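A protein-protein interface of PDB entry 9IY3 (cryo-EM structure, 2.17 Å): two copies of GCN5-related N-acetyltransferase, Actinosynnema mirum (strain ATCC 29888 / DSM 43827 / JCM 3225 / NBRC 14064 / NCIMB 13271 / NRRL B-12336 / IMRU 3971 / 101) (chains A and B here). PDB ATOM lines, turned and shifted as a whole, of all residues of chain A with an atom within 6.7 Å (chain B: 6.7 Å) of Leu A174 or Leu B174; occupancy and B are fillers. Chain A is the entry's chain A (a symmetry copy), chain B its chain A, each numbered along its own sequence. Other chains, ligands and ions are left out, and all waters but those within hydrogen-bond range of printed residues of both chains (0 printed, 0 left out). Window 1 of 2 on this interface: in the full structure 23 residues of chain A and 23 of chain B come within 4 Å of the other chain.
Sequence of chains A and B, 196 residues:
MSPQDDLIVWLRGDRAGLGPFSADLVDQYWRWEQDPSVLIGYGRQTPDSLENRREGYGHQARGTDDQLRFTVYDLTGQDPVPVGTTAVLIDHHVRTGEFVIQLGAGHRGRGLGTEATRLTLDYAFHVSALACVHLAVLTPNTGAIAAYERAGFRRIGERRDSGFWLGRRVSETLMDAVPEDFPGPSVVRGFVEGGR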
ATOM      1  N   HIS A 134      22.260  20.818 -31.182  1.00  0.00           N
ATOM      2  CA  HIS A 134      22.222  21.560 -29.932  1.00  0.00           C
ATOM      3  C   HIS A 134      23.441  21.222 -29.089  1.00  0.00           C
ATOM      4  O   HIS A 134      24.125  20.222 -29.315  1.00  0.00           O
ATOM      5  CB  HIS A 134      20.941  21.266 -29.141  1.00  0.00           C
ATOM      6  CG  HIS A 134      20.779  19.826 -28.767  1.00  0.00           C
ATOM      7  ND1 HIS A 134      21.289  19.300 -27.601  1.00  0.00           N
ATOM      8  CD2 HIS A 134      20.159  18.804 -29.402  1.00  0.00           C
ATOM      9  CE1 HIS A 134      20.995  18.014 -27.536  1.00  0.00           C
ATOM     10  NE2 HIS A 134      20.309  17.688 -28.615  1.00  0.00           N
ATOM     11  N   LEU A 135      23.713  22.085 -28.111  1.00  0.00           N
ATOM     12  CA  LEU A 135      24.839  21.897 -27.212  1.00  0.00           C
ATOM     13  C   LEU A 135      24.514  22.529 -25.868  1.00  0.00           C
ATOM     14  O   LEU A 135      23.608  23.357 -25.750  1.00  0.00           O
ATOM     15  CB  LEU A 135      26.132  22.486 -27.800  1.00  0.00           C
ATOM     16  CG  LEU A 135      26.221  23.978 -28.140  1.00  0.00           C
ATOM     17  CD1 LEU A 135      26.523  24.851 -26.930  1.00  0.00           C
ATOM     18  CD2 LEU A 135      27.262  24.200 -29.217  1.00  0.00           C
ATOM     19  N   ALA A 136      25.266  22.121 -24.851  1.00  0.00           N
ATOM     20  CA  ALA A 136      25.200  22.716 -23.525  1.00  0.00           C
ATOM     21  C   ALA A 136      26.593  23.182 -23.134  1.00  0.00           C
ATOM     22  O   ALA A 136      27.541  22.391 -23.144  1.00  0.00           O
ATOM     23  CB  ALA A 136      24.656  21.724 -22.496  1.00  0.00           C
ATOM     24  N   VAL A 137      26.713  24.460 -22.788  1.00  0.00           N
ATOM     25  CA  VAL A 137      27.999  25.073 -22.482  1.00  0.00           C
ATOM     26  C   VAL A 137      27.847  25.942 -21.241  1.00  0.00           C
ATOM     27  O   VAL A 137      26.825  26.609 -21.057  1.00  0.00           O
ATOM     28  CB  VAL A 137      28.535  25.882 -23.683  1.00  0.00           C
ATOM     29  CG1 VAL A 137      27.622  27.042 -23.997  1.00  0.00           C
ATOM     30  CG2 VAL A 137      29.944  26.376 -23.409  1.00  0.00           C
ATOM     31  N   ILE A 145      30.782  30.774 -26.236  1.00  0.00           N
ATOM     32  CA  ILE A 145      29.501  31.385 -26.588  1.00  0.00           C
ATOM     33  C   ILE A 145      29.630  32.179 -27.881  1.00  0.00           C
ATOM     34  O   ILE A 145      28.823  32.029 -28.806  1.00  0.00           O
ATOM     35  CB  ILE A 145      28.994  32.274 -25.439  1.00  0.00           C
ATOM     36  CG1 ILE A 145      28.674  31.438 -24.202  1.00  0.00           C
ATOM     37  CG2 ILE A 145      27.773  33.058 -25.877  1.00  0.00           C
ATOM     38  CD1 ILE A 145      27.514  30.513 -24.399  1.00  0.00           C
ATOM     39  N   ARG A 154      22.116  29.560 -31.851  1.00  0.00           N
ATOM     40  CA  ARG A 154      21.307  30.597 -31.231  1.00  0.00           C
ATOM     41  C   ARG A 154      21.009  30.207 -29.792  1.00  0.00           C
ATOM     42  O   ARG A 154      20.838  29.027 -29.475  1.00  0.00           O
ATOM     43  CB  ARG A 154      19.998  30.829 -31.995  1.00  0.00           C
ATOM     44  CG  ARG A 154      20.195  31.281 -33.429  1.00  0.00           C
ATOM     45  CD  ARG A 154      20.741  32.696 -33.493  1.00  0.00           C
ATOM     46  NE  ARG A 154      20.876  33.164 -34.867  1.00  0.00           N
ATOM     47  CZ  ARG A 154      21.972  33.026 -35.600  1.00  0.00           C
ATOM     48  NH1 ARG A 154      23.058  32.446 -35.118  1.00  0.00           N
ATOM     49  NH2 ARG A 154      21.979  33.484 -36.849  1.00  0.00           N
ATOM     50  N   ARG A 155      20.941  31.212 -28.926  1.00  0.00           N
ATOM     51  CA  ARG A 155      20.758  30.969 -27.502  1.00  0.00           C
ATOM     52  C   ARG A 155      19.319  30.561 -27.203  1.00  0.00           C
ATOM     53  O   ARG A 155      18.371  31.200 -27.668  1.00  0.00           O
ATOM     54  CB  ARG A 155      21.127  32.221 -26.708  1.00  0.00           C
ATOM     55  CG  ARG A 155      20.933  32.093 -25.210  1.00  0.00           C
ATOM     56  CD  ARG A 155      21.379  33.354 -24.489  1.00  0.00           C
ATOM     57  NE  ARG A 155      22.831  33.460 -24.399  1.00  0.00           N
ATOM     58  CZ  ARG A 155      23.565  34.294 -25.122  1.00  0.00           C
ATOM     59  NH1 ARG A 155      23.018  35.096 -26.019  1.00  0.00           N
ATOM     60  NH2 ARG A 155      24.881  34.325 -24.937  1.00  0.00           N
ATOM     61  N   ILE A 156      19.159  29.493 -26.427  1.00  0.00           N
ATOM     62  CA  ILE A 156      17.842  29.071 -25.956  1.00  0.00           C
ATOM     63  C   ILE A 156      17.531  29.663 -24.590  1.00  0.00           C
ATOM     64  O   ILE A 156      16.494  30.300 -24.395  1.00  0.00           O
ATOM     65  CB  ILE A 156      17.757  27.530 -25.920  1.00  0.00           C
ATOM     66  CG1 ILE A 156      17.938  26.938 -27.314  1.00  0.00           C
ATOM     67  CG2 ILE A 156      16.439  27.085 -25.315  1.00  0.00           C
ATOM     68  CD1 ILE A 156      18.159  25.445 -27.300  1.00  0.00           C
ATOM     69  N   GLY A 157      18.427  29.457 -23.634  1.00  0.00           N
ATOM     70  CA  GLY A 157      18.210  29.924 -22.282  1.00  0.00           C
ATOM     71  C   GLY A 157      19.282  29.372 -21.365  1.00  0.00           C
ATOM     72  O   GLY A 157      20.238  28.734 -21.809  1.00  0.00           O
ATOM     73  N   GLU A 158      19.101  29.630 -20.073  1.00  0.00           N
ATOM     74  CA  GLU A 158      20.059  29.234 -19.051  1.00  0.00           C
ATOM     75  C   GLU A 158      19.435  28.192 -18.135  1.00  0.00           C
ATOM     76  O   GLU A 158      18.347  28.408 -17.593  1.00  0.00           O
ATOM     77  CB  GLU A 158      20.520  30.446 -18.241  1.00  0.00           C
ATOM     78  CG  GLU A 158      21.582  31.282 -18.932  1.00  0.00           C
ATOM     79  CD  GLU A 158      21.993  32.494 -18.120  1.00  0.00           C
ATOM     80  OE1 GLU A 158      22.344  33.526 -18.728  1.00  0.00           O
ATOM     81  OE2 GLU A 158      21.965  32.415 -16.873  1.00  0.00           O
ATOM     82  N   ARG A 159      20.124  27.067 -17.965  1.00  0.00           N
ATOM     83  CA  ARG A 159      19.706  26.020 -17.039  1.00  0.00           C
ATOM     84  C   ARG A 159      20.368  26.295 -15.694  1.00  0.00           C
ATOM     85  O   ARG A 159      21.580  26.114 -15.542  1.00  0.00           O
ATOM     86  CB  ARG A 159      20.085  24.643 -17.573  1.00  0.00           C
ATOM     87  CG  ARG A 159      19.668  23.492 -16.680  1.00  0.00           C
ATOM     88  CD  ARG A 159      20.244  22.182 -17.183  1.00  0.00           C
ATOM     89  NE  ARG A 159      19.640  21.764 -18.442  1.00  0.00           N
ATOM     90  CZ  ARG A 159      20.214  20.938 -19.305  1.00  0.00           C
ATOM     91  NH1 ARG A 159      21.417  20.434 -19.085  1.00  0.00           N
ATOM     92  NH2 ARG A 159      19.566  20.613 -20.420  1.00  0.00           N
ATOM     93  N   GLU A 172      24.374  26.895 -17.060  1.00  0.00           N
ATOM     94  CA  GLU A 172      24.916  26.620 -18.382  1.00  0.00           C
ATOM     95  C   GLU A 172      23.930  27.085 -19.443  1.00  0.00           C
ATOM     96  O   GLU A 172      22.713  26.989 -19.263  1.00  0.00           O
ATOM     97  CB  GLU A 172      25.228  25.133 -18.573  1.00  0.00           C
ATOM     98  CG  GLU A 172      24.067  24.201 -18.322  1.00  0.00           C
ATOM     99  CD  GLU A 172      24.456  22.746 -18.492  1.00  0.00           C
ATOM    100  OE1 GLU A 172      25.662  22.469 -18.660  1.00  0.00           O
ATOM    101  OE2 GLU A 172      23.556  21.880 -18.466  1.00  0.00           O
ATOM    102  N   THR A 173      24.467  27.589 -20.550  1.00  0.00           N
ATOM    103  CA  THR A 173      23.655  28.125 -21.632  1.00  0.00           C
ATOM    104  C   THR A 173      23.355  27.029 -22.645  1.00  0.00           C
ATOM    105  O   THR A 173      24.262  26.319 -23.089  1.00  0.00           O
ATOM    106  CB  THR A 173      24.371  29.292 -22.313  1.00  0.00           C
ATOM    107  OG1 THR A 173      24.610  30.331 -21.356  1.00  0.00           O
ATOM    108  CG2 THR A 173      23.531  29.845 -23.449  1.00  0.00           C
ATOM    109  N   LEU A 174      22.084  26.894 -23.004  1.00  0.00           N
ATOM    110  CA  LEU A 174      21.648  25.933 -24.006  1.00  0.00           C
ATOM    111  C   LEU A 174      21.504  26.645 -25.343  1.00  0.00           C
ATOM    112  O   LEU A 174      20.901  27.720 -25.416  1.00  0.00           O
ATOM    113  CB  LEU A 174      20.325  25.282 -23.604  1.00  0.00           C
ATOM    114  CG  LEU A 174      20.267  24.656 -22.210  1.00  0.00           C
ATOM    115  CD1 LEU A 174      18.888  24.087 -21.938  1.00  0.00           C
ATOM    116  CD2 LEU A 174      21.329  23.584 -22.059  1.00  0.00           C
ATOM    117  N   MET A 175      22.069  26.054 -26.391  1.00  0.00           N
ATOM    118  CA  MET A 175      22.060  26.646 -27.718  1.00  0.00           C
ATOM    119  C   MET A 175      21.647  25.596 -28.739  1.00  0.00           C
ATOM    120  O   MET A 175      21.803  24.395 -28.512  1.00  0.00           O
ATOM    121  CB  MET A 175      23.435  27.220 -28.086  1.00  0.00           C
ATOM    122  CG  MET A 175      24.016  28.159 -27.043  1.00  0.00           C
ATOM    123  SD  MET A 175      25.602  28.859 -27.526  1.00  0.00           S
ATOM    124  CE  MET A 175      25.081  30.073 -28.731  1.00  0.00           C
ATOM    125  N   ASP A 176      21.109  26.062 -29.864  1.00  0.00           N
ATOM    126  CA  ASP A 176      20.706  25.166 -30.937  1.00  0.00           C
ATOM    127  C   ASP A 176      20.948  25.836 -32.281  1.00  0.00           C
ATOM    128  O   ASP A 176      21.096  27.057 -32.375  1.00  0.00           O
ATOM    129  CB  ASP A 176      19.239  24.726 -30.794  1.00  0.00           C
ATOM    130  CG  ASP A 176      18.259  25.893 -30.775  1.00  0.00           C
ATOM    131  OD1 ASP A 176      18.624  27.019 -31.167  1.00  0.00           O
ATOM    132  OD2 ASP A 176      17.099  25.674 -30.370  1.00  0.00           O
ATOM    133  N   HIS B 134      15.834  18.841 -14.216  1.00  0.00           N
ATOM    134  CA  HIS B 134      15.400  19.377 -15.495  1.00  0.00           C
ATOM    135  C   HIS B 134      14.706  18.293 -16.305  1.00  0.00           C
ATOM    136  O   HIS B 134      14.834  17.099 -16.027  1.00  0.00           O
ATOM    137  CB  HIS B 134      16.576  19.954 -16.293  1.00  0.00           C
ATOM    138  CG  HIS B 134      17.641  18.952 -16.610  1.00  0.00           C
ATOM    139  ND1 HIS B 134      17.614  18.173 -17.746  1.00  0.00           N
ATOM    140  CD2 HIS B 134      18.766  18.606 -15.943  1.00  0.00           C
ATOM    141  CE1 HIS B 134      18.674  17.386 -17.762  1.00  0.00           C
ATOM    142  NE2 HIS B 134      19.391  17.630 -16.680  1.00  0.00           N
ATOM    143  N   LEU B 135      13.954  18.730 -17.314  1.00  0.00           N
ATOM    144  CA  LEU B 135      13.234  17.817 -18.187  1.00  0.00           C
ATOM    145  C   LEU B 135      13.091  18.453 -19.560  1.00  0.00           C
ATOM    146  O   LEU B 135      13.243  19.665 -19.726  1.00  0.00           O
ATOM    147  CB  LEU B 135      11.861  17.448 -17.604  1.00  0.00           C
ATOM    148  CG  LEU B 135      10.818  18.536 -17.325  1.00  0.00           C
ATOM    149  CD1 LEU B 135      10.039  18.951 -18.566  1.00  0.00           C
ATOM    150  CD2 LEU B 135       9.866  18.072 -16.242  1.00  0.00           C
ATOM    151  N   ALA B 136      12.801  17.612 -20.548  1.00  0.00           N
ATOM    152  CA  ALA B 136      12.484  18.051 -21.898  1.00  0.00           C
ATOM    153  C   ALA B 136      11.129  17.483 -22.287  1.00  0.00           C
ATOM    154  O   ALA B 136      10.924  16.267 -22.230  1.00  0.00           O
ATOM    155  CB  ALA B 136      13.558  17.610 -22.894  1.00  0.00           C
ATOM    156  N   VAL B 137      10.212  18.359 -22.684  1.00  0.00           N
ATOM    157  CA  VAL B 137       8.841  17.975 -22.995  1.00  0.00           C
ATOM    158  C   VAL B 137       8.411  18.682 -24.274  1.00  0.00           C
ATOM    159  O   VAL B 137       8.756  19.845 -24.501  1.00  0.00           O
ATOM    160  CB  VAL B 137       7.890  18.290 -21.821  1.00  0.00           C
ATOM    161  CG1 VAL B 137       7.823  19.777 -21.569  1.00  0.00           C
ATOM    162  CG2 VAL B 137       6.503  17.737 -22.094  1.00  0.00           C
ATOM    163  N   ILE B 145       2.963  20.645 -19.439  1.00  0.00           N
ATOM    164  CA  ILE B 145       3.533  21.956 -19.132  1.00  0.00           C
ATOM    165  C   ILE B 145       2.899  22.528 -17.871  1.00  0.00           C
ATOM    166  O   ILE B 145       3.595  22.978 -16.953  1.00  0.00           O
ATOM    167  CB  ILE B 145       3.357  22.913 -20.325  1.00  0.00           C
ATOM    168  CG1 ILE B 145       4.163  22.435 -21.530  1.00  0.00           C
ATOM    169  CG2 ILE B 145       3.768  24.320 -19.938  1.00  0.00           C
ATOM    170  CD1 ILE B 145       5.643  22.497 -21.313  1.00  0.00           C
ATOM    171  N   ARG B 154      10.248  25.593 -13.912  1.00  0.00           N
ATOM    172  CA  ARG B 154      10.197  26.880 -14.586  1.00  0.00           C
ATOM    173  C   ARG B 154      10.699  26.719 -16.012  1.00  0.00           C
ATOM    174  O   ARG B 154      11.601  25.922 -16.282  1.00  0.00           O
ATOM    175  CB  ARG B 154      11.029  27.939 -13.853  1.00  0.00           C
ATOM    176  CG  ARG B 154      10.563  28.213 -12.436  1.00  0.00           C
ATOM    177  CD  ARG B 154       9.228  28.934 -12.422  1.00  0.00           C
ATOM    178  NE  ARG B 154       8.799  29.258 -11.067  1.00  0.00           N
ATOM    179  CZ  ARG B 154       8.046  28.470 -10.312  1.00  0.00           C
ATOM    180  NH1 ARG B 154       7.605  27.304 -10.753  1.00  0.00           N
ATOM    181  NH2 ARG B 154       7.723  28.865  -9.083  1.00  0.00           N
ATOM    182  N   ARG B 155      10.110  27.489 -16.920  1.00  0.00           N
ATOM    183  CA  ARG B 155      10.429  27.365 -18.336  1.00  0.00           C
ATOM    184  C   ARG B 155      11.792  27.979 -18.639  1.00  0.00           C
ATOM    185  O   ARG B 155      12.089  29.099 -18.215  1.00  0.00           O
ATOM    186  CB  ARG B 155       9.347  28.041 -19.175  1.00  0.00           C
ATOM    187  CG  ARG B 155       9.600  28.009 -20.669  1.00  0.00           C
ATOM    188  CD  ARG B 155       8.453  28.645 -21.435  1.00  0.00           C
ATOM    189  NE  ARG B 155       7.283  27.777 -21.507  1.00  0.00           N
ATOM    190  CZ  ARG B 155       6.171  27.962 -20.808  1.00  0.00           C
ATOM    191  NH1 ARG B 155       6.051  28.963 -19.953  1.00  0.00           N
ATOM    192  NH2 ARG B 155       5.154  27.122 -20.973  1.00  0.00           N
ATOM    193  N   ILE B 156      12.619  27.241 -19.372  1.00  0.00           N
ATOM    194  CA  ILE B 156      13.902  27.757 -19.846  1.00  0.00           C
ATOM    195  C   ILE B 156      13.774  28.352 -21.240  1.00  0.00           C
ATOM    196  O   ILE B 156      14.150  29.502 -21.477  1.00  0.00           O
ATOM    197  CB  ILE B 156      14.969  26.642 -19.820  1.00  0.00           C
ATOM    198  CG1 ILE B 156      15.195  26.134 -18.399  1.00  0.00           C
ATOM    199  CG2 ILE B 156      16.269  27.137 -20.426  1.00  0.00           C
ATOM    200  CD1 ILE B 156      15.999  24.857 -18.348  1.00  0.00           C
ATOM    201  N   GLY B 157      13.243  27.574 -22.173  1.00  0.00           N
ATOM    202  CA  GLY B 157      13.124  28.013 -23.546  1.00  0.00           C
ATOM    203  C   GLY B 157      12.682  26.859 -24.423  1.00  0.00           C
ATOM    204  O   GLY B 157      12.365  25.772 -23.938  1.00  0.00           O
ATOM    205  N   GLU B 158      12.672  27.119 -25.727  1.00  0.00           N
ATOM    206  CA  GLU B 158      12.218  26.154 -26.717  1.00  0.00           C
ATOM    207  C   GLU B 158      13.384  25.731 -27.599  1.00  0.00           C
ATOM    208  O   GLU B 158      14.078  26.580 -28.166  1.00  0.00           O
ATOM    209  CB  GLU B 158      11.092  26.740 -27.570  1.00  0.00           C
ATOM    210  CG  GLU B 158       9.731  26.711 -26.898  1.00  0.00           C
ATOM    211  CD  GLU B 158       8.644  27.330 -27.752  1.00  0.00           C
ATOM    212  OE1 GLU B 158       7.696  27.909 -27.183  1.00  0.00           O
ATOM    213  OE2 GLU B 158       8.735  27.236 -28.995  1.00  0.00           O
ATOM    214  N   ARG B 159      13.594  24.422 -27.711  1.00  0.00           N
ATOM    215  CA  ARG B 159      14.607  23.862 -28.599  1.00  0.00           C
ATOM    216  C   ARG B 159      13.946  23.585 -29.945  1.00  0.00           C
ATOM    217  O   ARG B 159      13.146  22.652 -30.070  1.00  0.00           O
ATOM    218  CB  ARG B 159      15.207  22.593 -28.003  1.00  0.00           C
ATOM    219  CG  ARG B 159      16.285  21.954 -28.854  1.00  0.00           C
ATOM    220  CD  ARG B 159      16.692  20.607 -28.288  1.00  0.00           C
ATOM    221  NE  ARG B 159      17.404  20.735 -27.023  1.00  0.00           N
ATOM    222  CZ  ARG B 159      17.492  19.771 -26.117  1.00  0.00           C
ATOM    223  NH1 ARG B 159      16.909  18.597 -26.298  1.00  0.00           N
ATOM    224  NH2 ARG B 159      18.178  19.992 -25.000  1.00  0.00           N
ATOM    225  N   GLU B 172      10.493  21.490 -28.543  1.00  0.00           N
ATOM    226  CA  GLU B 172      10.239  20.985 -27.203  1.00  0.00           C
ATOM    227  C   GLU B 172      10.669  22.022 -26.177  1.00  0.00           C
ATOM    228  O   GLU B 172      11.659  22.733 -26.372  1.00  0.00           O
ATOM    229  CB  GLU B 172      10.967  19.661 -26.946  1.00  0.00           C
ATOM    230  CG  GLU B 172      12.459  19.699 -27.175  1.00  0.00           C
ATOM    231  CD  GLU B 172      13.107  18.350 -26.939  1.00  0.00           C
ATOM    232  OE1 GLU B 172      12.368  17.362 -26.741  1.00  0.00           O
ATOM    233  OE2 GLU B 172      14.354  18.276 -26.943  1.00  0.00           O
ATOM    234  N   THR B 173       9.917  22.101 -25.084  1.00  0.00           N
ATOM    235  CA  THR B 173      10.168  23.080 -24.038  1.00  0.00           C
ATOM    236  C   THR B 173      11.094  22.486 -22.985  1.00  0.00           C
ATOM    237  O   THR B 173      10.860  21.376 -22.498  1.00  0.00           O
ATOM    238  CB  THR B 173       8.855  23.528 -23.394  1.00  0.00           C
ATOM    239  OG1 THR B 173       8.013  24.121 -24.390  1.00  0.00           O
ATOM    240  CG2 THR B 173       9.116  24.541 -22.296  1.00  0.00           C
ATOM    241  N   LEU B 174      12.141  23.226 -22.640  1.00  0.00           N
ATOM    242  CA  LEU B 174      13.082  22.821 -21.606  1.00  0.00           C
ATOM    243  C   LEU B 174      12.708  23.511 -20.302  1.00  0.00           C
ATOM    244  O   LEU B 174      12.466  24.721 -20.283  1.00  0.00           O
ATOM    245  CB  LEU B 174      14.516  23.171 -22.001  1.00  0.00           C
ATOM    246  CG  LEU B 174      14.988  22.677 -23.368  1.00  0.00           C
ATOM    247  CD1 LEU B 174      16.411  23.130 -23.637  1.00  0.00           C
ATOM    248  CD2 LEU B 174      14.882  21.167 -23.458  1.00  0.00           C
ATOM    249  N   MET B 175      12.648  22.738 -19.222  1.00  0.00           N
ATOM    250  CA  MET B 175      12.249  23.247 -17.921  1.00  0.00           C
ATOM    251  C   MET B 175      13.230  22.763 -16.864  1.00  0.00           C
ATOM    252  O   MET B 175      13.896  21.740 -17.039  1.00  0.00           O
ATOM    253  CB  MET B 175      10.825  22.804 -17.556  1.00  0.00           C
ATOM    254  CG  MET B 175       9.789  23.096 -18.628  1.00  0.00           C
ATOM    255  SD  MET B 175       8.123  22.615 -18.150  1.00  0.00           S
ATOM    256  CE  MET B 175       7.710  23.925 -17.004  1.00  0.00           C
ATOM    257  N   ASP B 176      13.318  23.512 -15.768  1.00  0.00           N
ATOM    258  CA  ASP B 176      14.191  23.139 -14.664  1.00  0.00           C
ATOM    259  C   ASP B 176      13.550  23.545 -13.345  1.00  0.00           C
ATOM    260  O   ASP B 176      12.642  24.380 -13.300  1.00  0.00           O
ATOM    261  CB  ASP B 176      15.593  23.753 -14.811  1.00  0.00           C
ATOM    262  CG  ASP B 176      15.578  25.275 -14.893  1.00  0.00           C
ATOM    263  OD1 ASP B 176      14.562  25.908 -14.543  1.00  0.00           O
ATOM    264  OD2 ASP B 176      16.607  25.847 -15.307  1.00  0.00           O
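His A134 touches Arg B159, and with the chains exchanged Arg A159 touches His B134.
Ile B156 touches its own counterpart, Ile A156.
Ile A156 touches Gly B157, and with the chains exchanged Gly A157 touches Ile B156.
Ile A156 touches Glu B158, and with the chains exchanged Glu A158 touches Ile B156.
Hydrophobic or aromatic side chains of chain A within 4 Å of the printed part of chain B: His A134, Ile A156 and Leu A174.
Of the 16 printed residues of chain B, 7 touch a printed residue of chain A.
Hydrophobic or aromatic side chains of chain B within 4 Å of the printed part of chain A: His B134, Ile B156 and Leu B174.
Among the printed residues, 12 pairs touch across the chains.
Among the printed residues, no Asp or Glu carboxylate lies within 4 Å of a Lys or Arg side-chain nitrogen of the other chain.
Of the printed residues of chain B, Ile A156 touches Ile B156 (3.8 Å), Gly B157 (3.9 Å) and Glu B158 (3.7 Å).
Printed residues of chain B within 4 Å of Glu A158: Ile B156 (3.7 Å) and Asp B176 (3.8 Å).
Of the printed residues of chain B, Arg A159 touches His B134 (3.9 Å) and Asp B176 (3.6 Å).
Leu A174 touches one residue of chain B.
Of the printed residues of chain A, Gly B157 touches Ile A156 (3.9 Å).
Of the printed residues of chain A, Arg B159 touches His A134 (3.9 Å) and Asp A176 (3.6 Å).
O of Asp B176 sits at hydrogen-bond distance from N of Arg B154.
The backbone carbonyl oxygen (O) of Gly B157 sits at hydrogen-bond distance from the backbone NH (N) of Leu B174, at 2.9 Å.
The guanidinium group of Arg B159 lies within salt-bridge range of the side-chain carboxylate of Glu B172, at 2.7 Å.
The backbone carbonyl oxygen (O) of Asp A176 is in hydrogen-bond range of the backbone NH (N) of Arg A154 (2.8 Å).
O of Gly A157 is in hydrogen-bond range of N of Leu A174.
The guanidinium group (NH1) of Arg A159 is in salt-bridge range of the side-chain carboxylate (OE2) of Glu A172, 2.7 Å away.
Arg B159 touches His A134 (NE to CG, 3.9 Å).
Ile B156 touches Ile A156.
Ile A156 touches Gly B157.
Ile A156 touches Glu B158 (CG2 to O, 3.7 Å).
Gly A157 touches Ile B156 (C to CG2, 3.9 Å).
O of Glu A158 touches CG2 of Ile B156 (3.7 Å).
His B134 touches Arg A159.
Leu B174 touches Leu A174 (CD1 to CD1, 3.2 Å).
Asp A176 touches Glu B158.
Arg B159 touches Asp A176.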
